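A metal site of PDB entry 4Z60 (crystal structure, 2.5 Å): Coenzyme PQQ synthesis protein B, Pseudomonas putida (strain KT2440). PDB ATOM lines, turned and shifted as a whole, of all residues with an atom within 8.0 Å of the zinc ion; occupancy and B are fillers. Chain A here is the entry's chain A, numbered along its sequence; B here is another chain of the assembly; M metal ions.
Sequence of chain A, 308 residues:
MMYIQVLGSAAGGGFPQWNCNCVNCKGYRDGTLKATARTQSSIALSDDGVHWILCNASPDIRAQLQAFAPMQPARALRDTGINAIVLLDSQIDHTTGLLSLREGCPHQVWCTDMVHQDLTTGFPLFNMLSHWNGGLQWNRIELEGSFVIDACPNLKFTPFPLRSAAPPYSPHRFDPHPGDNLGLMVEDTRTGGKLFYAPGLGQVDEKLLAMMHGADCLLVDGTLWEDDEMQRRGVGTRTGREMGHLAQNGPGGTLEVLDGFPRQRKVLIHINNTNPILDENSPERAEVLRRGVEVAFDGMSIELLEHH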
ATOM      1  N   GLY A  14      13.936  -9.587  30.084  1.00  0.00           N
ATOM      2  CA  GLY A  14      12.950  -9.946  29.083  1.00  0.00           C
ATOM      3  C   GLY A  14      13.549 -10.755  27.938  1.00  0.00           C
ATOM      4  O   GLY A  14      14.700 -11.171  27.996  1.00  0.00           O
ATOM      5  N   PHE A  15      12.736 -10.996  26.916  1.00  0.00           N
ATOM      6  CA  PHE A  15      13.228 -11.605  25.680  1.00  0.00           C
ATOM      7  C   PHE A  15      12.557 -10.974  24.466  1.00  0.00           C
ATOM      8  O   PHE A  15      11.336 -11.038  24.329  1.00  0.00           O
ATOM      9  CB  PHE A  15      13.017 -13.118  25.665  1.00  0.00           C
ATOM     10  CG  PHE A  15      13.351 -13.748  24.343  1.00  0.00           C
ATOM     11  CD1 PHE A  15      14.668 -13.793  23.908  1.00  0.00           C
ATOM     12  CD2 PHE A  15      12.362 -14.277  23.535  1.00  0.00           C
ATOM     13  CE1 PHE A  15      14.985 -14.357  22.691  1.00  0.00           C
ATOM     14  CE2 PHE A  15      12.679 -14.840  22.318  1.00  0.00           C
ATOM     15  CZ  PHE A  15      13.993 -14.882  21.891  1.00  0.00           C
ATOM     16  N   PRO A  16      13.361 -10.367  23.577  1.00  0.00           N
ATOM     17  CA  PRO A  16      14.821 -10.253  23.705  1.00  0.00           C
ATOM     18  C   PRO A  16      15.235  -9.219  24.750  1.00  0.00           C
ATOM     19  O   PRO A  16      14.437  -8.350  25.114  1.00  0.00           O
ATOM     20  CB  PRO A  16      15.236  -9.769  22.316  1.00  0.00           C
ATOM     21  CG  PRO A  16      14.055  -8.995  21.824  1.00  0.00           C
ATOM     22  CD  PRO A  16      12.852  -9.738  22.342  1.00  0.00           C
ATOM     23  N   GLN A  17      16.467  -9.331  25.231  1.00  0.00           N
ATOM     24  CA  GLN A  17      17.003  -8.358  26.180  1.00  0.00           C
ATOM     25  C   GLN A  17      17.569  -7.162  25.408  1.00  0.00           C
ATOM     26  O   GLN A  17      18.234  -7.336  24.377  1.00  0.00           O
ATOM     27  CB  GLN A  17      18.071  -9.003  27.072  1.00  0.00           C
ATOM     28  CG  GLN A  17      18.543  -8.139  28.219  1.00  0.00           C
ATOM     29  CD  GLN A  17      19.358  -8.923  29.247  1.00  0.00           C
ATOM     30  OE1 GLN A  17      18.874  -9.869  29.851  1.00  0.00           O
ATOM     31  NE2 GLN A  17      20.620  -8.520  29.429  1.00  0.00           N
ATOM     32  N   TRP A  18      17.286  -5.970  25.910  1.00  0.00           N
ATOM     33  CA  TRP A  18      17.581  -4.724  25.205  1.00  0.00           C
ATOM     34  C   TRP A  18      19.021  -4.611  24.708  1.00  0.00           C
ATOM     35  O   TRP A  18      19.274  -4.058  23.641  1.00  0.00           O
ATOM     36  CB  TRP A  18      17.262  -3.512  26.097  1.00  0.00           C
ATOM     37  CG  TRP A  18      18.164  -3.422  27.298  1.00  0.00           C
ATOM     38  CD1 TRP A  18      18.053  -4.118  28.470  1.00  0.00           C
ATOM     39  CD2 TRP A  18      19.312  -2.583  27.436  1.00  0.00           C
ATOM     40  NE1 TRP A  18      19.070  -3.768  29.323  1.00  0.00           N
ATOM     41  CE2 TRP A  18      19.859  -2.819  28.715  1.00  0.00           C
ATOM     42  CE3 TRP A  18      19.940  -1.648  26.594  1.00  0.00           C
ATOM     43  CZ2 TRP A  18      20.994  -2.171  29.180  1.00  0.00           C
ATOM     44  CZ3 TRP A  18      21.074  -1.000  27.060  1.00  0.00           C
ATOM     45  CH2 TRP A  18      21.591  -1.267  28.339  1.00  0.00           C
ATOM     46  N   ASN A  19      19.971  -5.145  25.473  1.00  0.00           N
ATOM     47  CA  ASN A  19      21.381  -5.016  25.146  1.00  0.00           C
ATOM     48  C   ASN A  19      22.055  -6.320  24.694  1.00  0.00           C
ATOM     49  O   ASN A  19      23.269  -6.355  24.504  1.00  0.00           O
ATOM     50  CB  ASN A  19      22.152  -4.412  26.331  1.00  0.00           C
ATOM     51  CG  ASN A  19      22.240  -5.359  27.516  1.00  0.00           C
ATOM     52  OD1 ASN A  19      21.344  -6.177  27.756  1.00  0.00           O
ATOM     53  ND2 ASN A  19      23.323  -5.255  28.283  1.00  0.00           N
ATOM     54  N   CYS A  20      21.263  -7.366  24.525  1.00  0.00           N
ATOM     55  CA  CYS A  20      21.804  -8.699  24.239  1.00  0.00           C
ATOM     56  C   CYS A  20      21.728  -9.115  22.765  1.00  0.00           C
ATOM     57  O   CYS A  20      20.719  -8.923  22.102  1.00  0.00           O
ATOM     58  CB  CYS A  20      21.115  -9.753  25.094  1.00  0.00           C
ATOM     59  SG  CYS A  20      21.802 -11.404  24.885  1.00  0.00           S
ATOM     60  N   ASN A  21      22.807  -9.712  22.278  1.00  0.00           N
ATOM     61  CA  ASN A  21      22.833 -10.262  20.922  1.00  0.00           C
ATOM     62  C   ASN A  21      23.271 -11.716  20.904  1.00  0.00           C
ATOM     63  O   ASN A  21      23.982 -12.138  19.992  1.00  0.00           O
ATOM     64  CB  ASN A  21      23.757  -9.445  20.019  1.00  0.00           C
ATOM     65  CG  ASN A  21      23.318  -7.999  19.910  1.00  0.00           C
ATOM     66  OD1 ASN A  21      22.328  -7.675  19.256  1.00  0.00           O
ATOM     67  ND2 ASN A  21      24.074  -7.103  20.555  1.00  0.00           N
ATOM     68  N   CYS A  22      22.846 -12.485  21.906  1.00  0.00           N
ATOM     69  CA  CYS A  22      23.150 -13.905  21.941  1.00  0.00           C
ATOM     70  C   CYS A  22      22.386 -14.596  20.810  1.00  0.00           C
ATOM     71  O   CYS A  22      21.612 -13.948  20.098  1.00  0.00           O
ATOM     72  CB  CYS A  22      22.761 -14.515  23.292  1.00  0.00           C
ATOM     73  SG  CYS A  22      20.979 -14.762  23.515  1.00  0.00           S
ATOM     74  N   VAL A  23      22.592 -15.905  20.645  1.00  0.00           N
ATOM     75  CA  VAL A  23      21.966 -16.624  19.553  1.00  0.00           C
ATOM     76  C   VAL A  23      20.436 -16.439  19.509  1.00  0.00           C
ATOM     77  O   VAL A  23      19.870 -16.236  18.437  1.00  0.00           O
ATOM     78  CB  VAL A  23      22.341 -18.125  19.539  1.00  0.00           C
ATOM     79  CG1 VAL A  23      23.855 -18.294  19.462  1.00  0.00           C
ATOM     80  CG2 VAL A  23      21.798 -18.839  20.759  1.00  0.00           C
ATOM     81  N   ASN A  24      19.787 -16.463  20.670  1.00  0.00           N
ATOM     82  CA  ASN A  24      18.342 -16.274  20.734  1.00  0.00           C
ATOM     83  C   ASN A  24      17.894 -14.847  20.416  1.00  0.00           C
ATOM     84  O   ASN A  24      17.069 -14.636  19.520  1.00  0.00           O
ATOM     85  CB  ASN A  24      17.798 -16.688  22.105  1.00  0.00           C
ATOM     86  CG  ASN A  24      17.779 -18.196  22.306  1.00  0.00           C
ATOM     87  OD1 ASN A  24      17.894 -18.971  21.351  1.00  0.00           O
ATOM     88  ND2 ASN A  24      17.626 -18.621  23.551  1.00  0.00           N
ATOM     89  N   CYS A  25      18.441 -13.871  21.132  1.00  0.00           N
ATOM     90  CA  CYS A  25      18.036 -12.469  20.976  1.00  0.00           C
ATOM     91  C   CYS A  25      18.300 -11.923  19.573  1.00  0.00           C
ATOM     92  O   CYS A  25      17.457 -11.247  18.994  1.00  0.00           O
ATOM     93  CB  CYS A  25      18.715 -11.580  22.015  1.00  0.00           C
ATOM     94  SG  CYS A  25      18.197 -11.885  23.718  1.00  0.00           S
ATOM     95  N   LYS A  26      19.491 -12.211  19.046  1.00  0.00           N
ATOM     96  CA  LYS A  26      19.848 -11.741  17.719  1.00  0.00           C
ATOM     97  C   LYS A  26      19.070 -12.508  16.662  1.00  0.00           C
ATOM     98  O   LYS A  26      18.650 -11.951  15.642  1.00  0.00           O
ATOM     99  CB  LYS A  26      21.357 -11.871  17.492  1.00  0.00           C
ATOM    100  CG  LYS A  26      21.833 -11.379  16.138  1.00  0.00           C
ATOM    101  CD  LYS A  26      23.345 -11.515  16.034  1.00  0.00           C
ATOM    102  CE  LYS A  26      23.820 -11.192  14.636  1.00  0.00           C
ATOM    103  NZ  LYS A  26      23.447  -9.808  14.253  1.00  0.00           N
ATOM    104  N   GLY A  27      18.859 -13.794  16.914  1.00  0.00           N
ATOM    105  CA  GLY A  27      18.113 -14.646  16.004  1.00  0.00           C
ATOM    106  C   GLY A  27      16.659 -14.236  15.918  1.00  0.00           C
ATOM    107  O   GLY A  27      16.033 -14.314  14.861  1.00  0.00           O
ATOM    108  N   ARG A  29      15.543 -11.063  16.475  1.00  0.00           N
ATOM    109  CA  ARG A  29      15.542  -9.799  15.746  1.00  0.00           C
ATOM    110  C   ARG A  29      15.763  -9.982  14.245  1.00  0.00           C
ATOM    111  O   ARG A  29      15.236  -9.220  13.440  1.00  0.00           O
ATOM    112  CB  ARG A  29      16.607  -8.851  16.295  1.00  0.00           C
ATOM    113  CG  ARG A  29      16.362  -8.393  17.723  1.00  0.00           C
ATOM    114  CD  ARG A  29      17.326  -7.271  18.089  1.00  0.00           C
ATOM    115  NE  ARG A  29      17.299  -6.972  19.521  1.00  0.00           N
ATOM    116  CZ  ARG A  29      18.176  -7.456  20.397  1.00  0.00           C
ATOM    117  NH1 ARG A  29      18.080  -7.125  21.676  1.00  0.00           N
ATOM    118  NH2 ARG A  29      19.152  -8.251  19.986  1.00  0.00           N
ATOM    119  N   MET A 230      25.346 -18.541  30.839  1.00  0.00           N
ATOM    120  CA  MET A 230      25.821 -17.199  30.517  1.00  0.00           C
ATOM    121  C   MET A 230      27.215 -17.229  29.897  1.00  0.00           C
ATOM    122  O   MET A 230      27.539 -16.400  29.047  1.00  0.00           O
ATOM    123  CB  MET A 230      25.795 -16.306  31.756  1.00  0.00           C
ATOM    124  CG  MET A 230      24.391 -15.994  32.269  1.00  0.00           C
ATOM    125  SD  MET A 230      23.416 -14.978  31.136  1.00  0.00           S
ATOM    126  CE  MET A 230      24.266 -13.407  31.251  1.00  0.00           C
ATOM    127  N   ARG A 233      26.906 -18.673  26.119  1.00  0.00           N
ATOM    128  CA  ARG A 233      26.401 -17.691  25.167  1.00  0.00           C
ATOM    129  C   ARG A 233      27.420 -16.567  24.965  1.00  0.00           C
ATOM    130  O   ARG A 233      27.385 -15.856  23.956  1.00  0.00           O
ATOM    131  CB  ARG A 233      25.068 -17.109  25.641  1.00  0.00           C
ATOM    132  CG  ARG A 233      24.046 -18.162  26.047  1.00  0.00           C
ATOM    133  CD  ARG A 233      23.988 -19.283  25.025  1.00  0.00           C
ATOM    134  NE  ARG A 233      22.644 -19.846  24.913  1.00  0.00           N
ATOM    135  CZ  ARG A 233      22.202 -20.532  23.867  1.00  0.00           C
ATOM    136  NH1 ARG A 233      20.965 -21.011  23.848  1.00  0.00           N
ATOM    137  NH2 ARG A 233      23.003 -20.732  22.827  1.00  0.00           N
ATOM    138  N   VAL A 235      27.887 -13.976  27.142  1.00  0.00           N
ATOM    139  CA  VAL A 235      27.285 -12.693  27.530  1.00  0.00           C
ATOM    140  C   VAL A 235      27.339 -12.416  29.032  1.00  0.00           C
ATOM    141  O   VAL A 235      26.679 -11.508  29.525  1.00  0.00           O
ATOM    142  CB  VAL A 235      25.818 -12.605  27.072  1.00  0.00           C
ATOM    143  CG1 VAL A 235      25.737 -12.574  25.550  1.00  0.00           C
ATOM    144  CG2 VAL A 235      25.013 -13.769  27.626  1.00  0.00           C
ATOM    145  N   ASN A 272      15.239 -17.220  30.934  1.00  0.00           N
ATOM    146  CA  ASN A 272      16.208 -16.233  30.486  1.00  0.00           C
ATOM    147  C   ASN A 272      16.335 -16.190  28.959  1.00  0.00           C
ATOM    148  O   ASN A 272      16.142 -17.201  28.290  1.00  0.00           O
ATOM    149  CB  ASN A 272      17.586 -16.495  31.111  1.00  0.00           C
ATOM    150  CG  ASN A 272      18.445 -15.253  31.163  1.00  0.00           C
ATOM    151  OD1 ASN A 272      17.988 -14.186  31.559  1.00  0.00           O
ATOM    152  ND2 ASN A 272      19.701 -15.377  30.735  1.00  0.00           N
ATOM    153  N   ASN A 273      16.669 -15.015  28.434  1.00  0.00           N
ATOM    154  CA  ASN A 273      16.811 -14.817  27.000  1.00  0.00           C
ATOM    155  C   ASN A 273      17.840 -15.763  26.360  1.00  0.00           C
ATOM    156  O   ASN A 273      17.809 -15.997  25.158  1.00  0.00           O
ATOM    157  CB  ASN A 273      17.184 -13.373  26.693  1.00  0.00           C
ATOM    158  CG  ASN A 273      18.552 -12.981  27.272  1.00  0.00           C
ATOM    159  OD1 ASN A 273      19.585 -13.199  26.642  1.00  0.00           O
ATOM    160  ND2 ASN A 273      18.545 -12.418  28.477  1.00  0.00           N
ATOM    161  N   THR A 274      18.746 -16.295  27.176  1.00  0.00           N
ATOM    162  CA  THR A 274      19.791 -17.180  26.694  1.00  0.00           C
ATOM    163  C   THR A 274      19.362 -18.643  26.593  1.00  0.00           C
ATOM    164  O   THR A 274      20.064 -19.462  26.009  1.00  0.00           O
ATOM    165  CB  THR A 274      21.052 -17.086  27.583  1.00  0.00           C
ATOM    166  OG1 THR A 274      20.693 -17.325  28.948  1.00  0.00           O
ATOM    167  CG2 THR A 274      21.704 -15.704  27.454  1.00  0.00           C
ATOM    168  N   ASN A 275      18.200 -18.966  27.168  1.00  0.00           N
ATOM    169  CA  ASN A 275      17.759 -20.349  27.262  1.00  0.00           C
ATOM    170  C   ASN A 275      17.315 -20.927  25.918  1.00  0.00           C
ATOM    171  O   ASN A 275      16.438 -20.368  25.258  1.00  0.00           O
ATOM    172  CB  ASN A 275      16.628 -20.468  28.294  1.00  0.00           C
ATOM    173  CG  ASN A 275      16.438 -21.899  28.808  1.00  0.00           C
ATOM    174  OD1 ASN A 275      16.606 -22.871  28.073  1.00  0.00           O
ATOM    175  ND2 ASN A 275      16.074 -22.022  30.085  1.00  0.00           N
ATOM    176  N   LEU A 278      13.688 -21.492  24.458  1.00  0.00           N
ATOM    177  CA  LEU A 278      12.996 -20.405  23.777  1.00  0.00           C
ATOM    178  C   LEU A 278      12.962 -20.662  22.276  1.00  0.00           C
ATOM    179  O   LEU A 278      11.998 -20.295  21.602  1.00  0.00           O
ATOM    180  CB  LEU A 278      13.661 -19.062  24.063  1.00  0.00           C
ATOM    181  CG  LEU A 278      13.496 -18.574  25.502  1.00  0.00           C
ATOM    182  CD1 LEU A 278      14.021 -17.148  25.640  1.00  0.00           C
ATOM    183  CD2 LEU A 278      12.043 -18.662  25.923  1.00  0.00           C
ATOM    184  N   LEU B  77      28.298  -9.189  21.535  1.00  0.00           N
ATOM    185  CA  LEU B  77      27.295 -10.005  22.212  1.00  0.00           C
ATOM    186  C   LEU B  77      26.471  -9.189  23.216  1.00  0.00           C
ATOM    187  O   LEU B  77      25.310  -9.498  23.477  1.00  0.00           O
ATOM    188  CB  LEU B  77      27.959 -11.193  22.901  1.00  0.00           C
ATOM    189  CG  LEU B  77      28.630 -12.136  21.896  1.00  0.00           C
ATOM    190  CD1 LEU B  77      29.249 -13.330  22.590  1.00  0.00           C
ATOM    191  CD2 LEU B  77      27.616 -12.576  20.847  1.00  0.00           C
ATOM    192  N   ARG B  78      27.095  -8.149  23.761  1.00  0.00           N
ATOM    193  CA  ARG B  78      26.377  -7.156  24.557  1.00  0.00           C
ATOM    194  C   ARG B  78      26.729  -5.767  24.028  1.00  0.00           C
ATOM    195  O   ARG B  78      27.892  -5.401  23.909  1.00  0.00           O
ATOM    196  CB  ARG B  78      26.688  -7.308  26.046  1.00  0.00           C
ATOM    197  CG  ARG B  78      26.049  -8.549  26.688  1.00  0.00           C
ATOM    198  CD  ARG B  78      24.550  -8.358  26.880  1.00  0.00           C
ATOM    199  NE  ARG B  78      23.827  -9.619  27.052  1.00  0.00           N
ATOM    200  CZ  ARG B  78      23.461 -10.128  28.227  1.00  0.00           C
ATOM    201  NH1 ARG B  78      23.752  -9.484  29.353  1.00  0.00           N
ATOM    202  NH2 ARG B  78      22.800 -11.270  28.280  1.00  0.00           N
HETATM  203 ZN    ZN M   1      20.089 -12.867  24.602  1.00  0.00          ZN
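The nearest printed residue that does not touch the zinc ion is Thr 274 (4.3 Å).
OD1 of Asn 273 is bound to the zinc ion (2.1 Å).
The zinc ion is bound by SG of Cys 20 (2.3 Å).
SG of Cys 25 is bound to the zinc ion (2.3 Å).
The zinc ion is bound by SG of Cys 22, 2.4 Å away.
The zinc ion has four donor atoms within binding distance.
The side-chain amide oxygen of Gln 17 lies within hydrogen-bond range of the side-chain amide nitrogen of Asn 273.
O of Asn 273 is in hydrogen-bond range of ND2 of Asn 24, at 3.1 Å.
The side-chain sulfur (SG) of Cys 20 sits close to the guanidinium group (NE) of Arg 78 of chain B (3.5 Å).
The guanidinium group (NH2) of Arg 29 sits at hydrogen-bond distance from the backbone carbonyl oxygen (O) of Cys 20 (2.7 Å).
The backbone NH of Gln 17 lies close to the side-chain sulfur of Cys 25 (3.4 Å).
The side-chain sulfur (SG) of Cys 22 sits close to the backbone NH (N) of Asn 24, at 3.5 Å.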
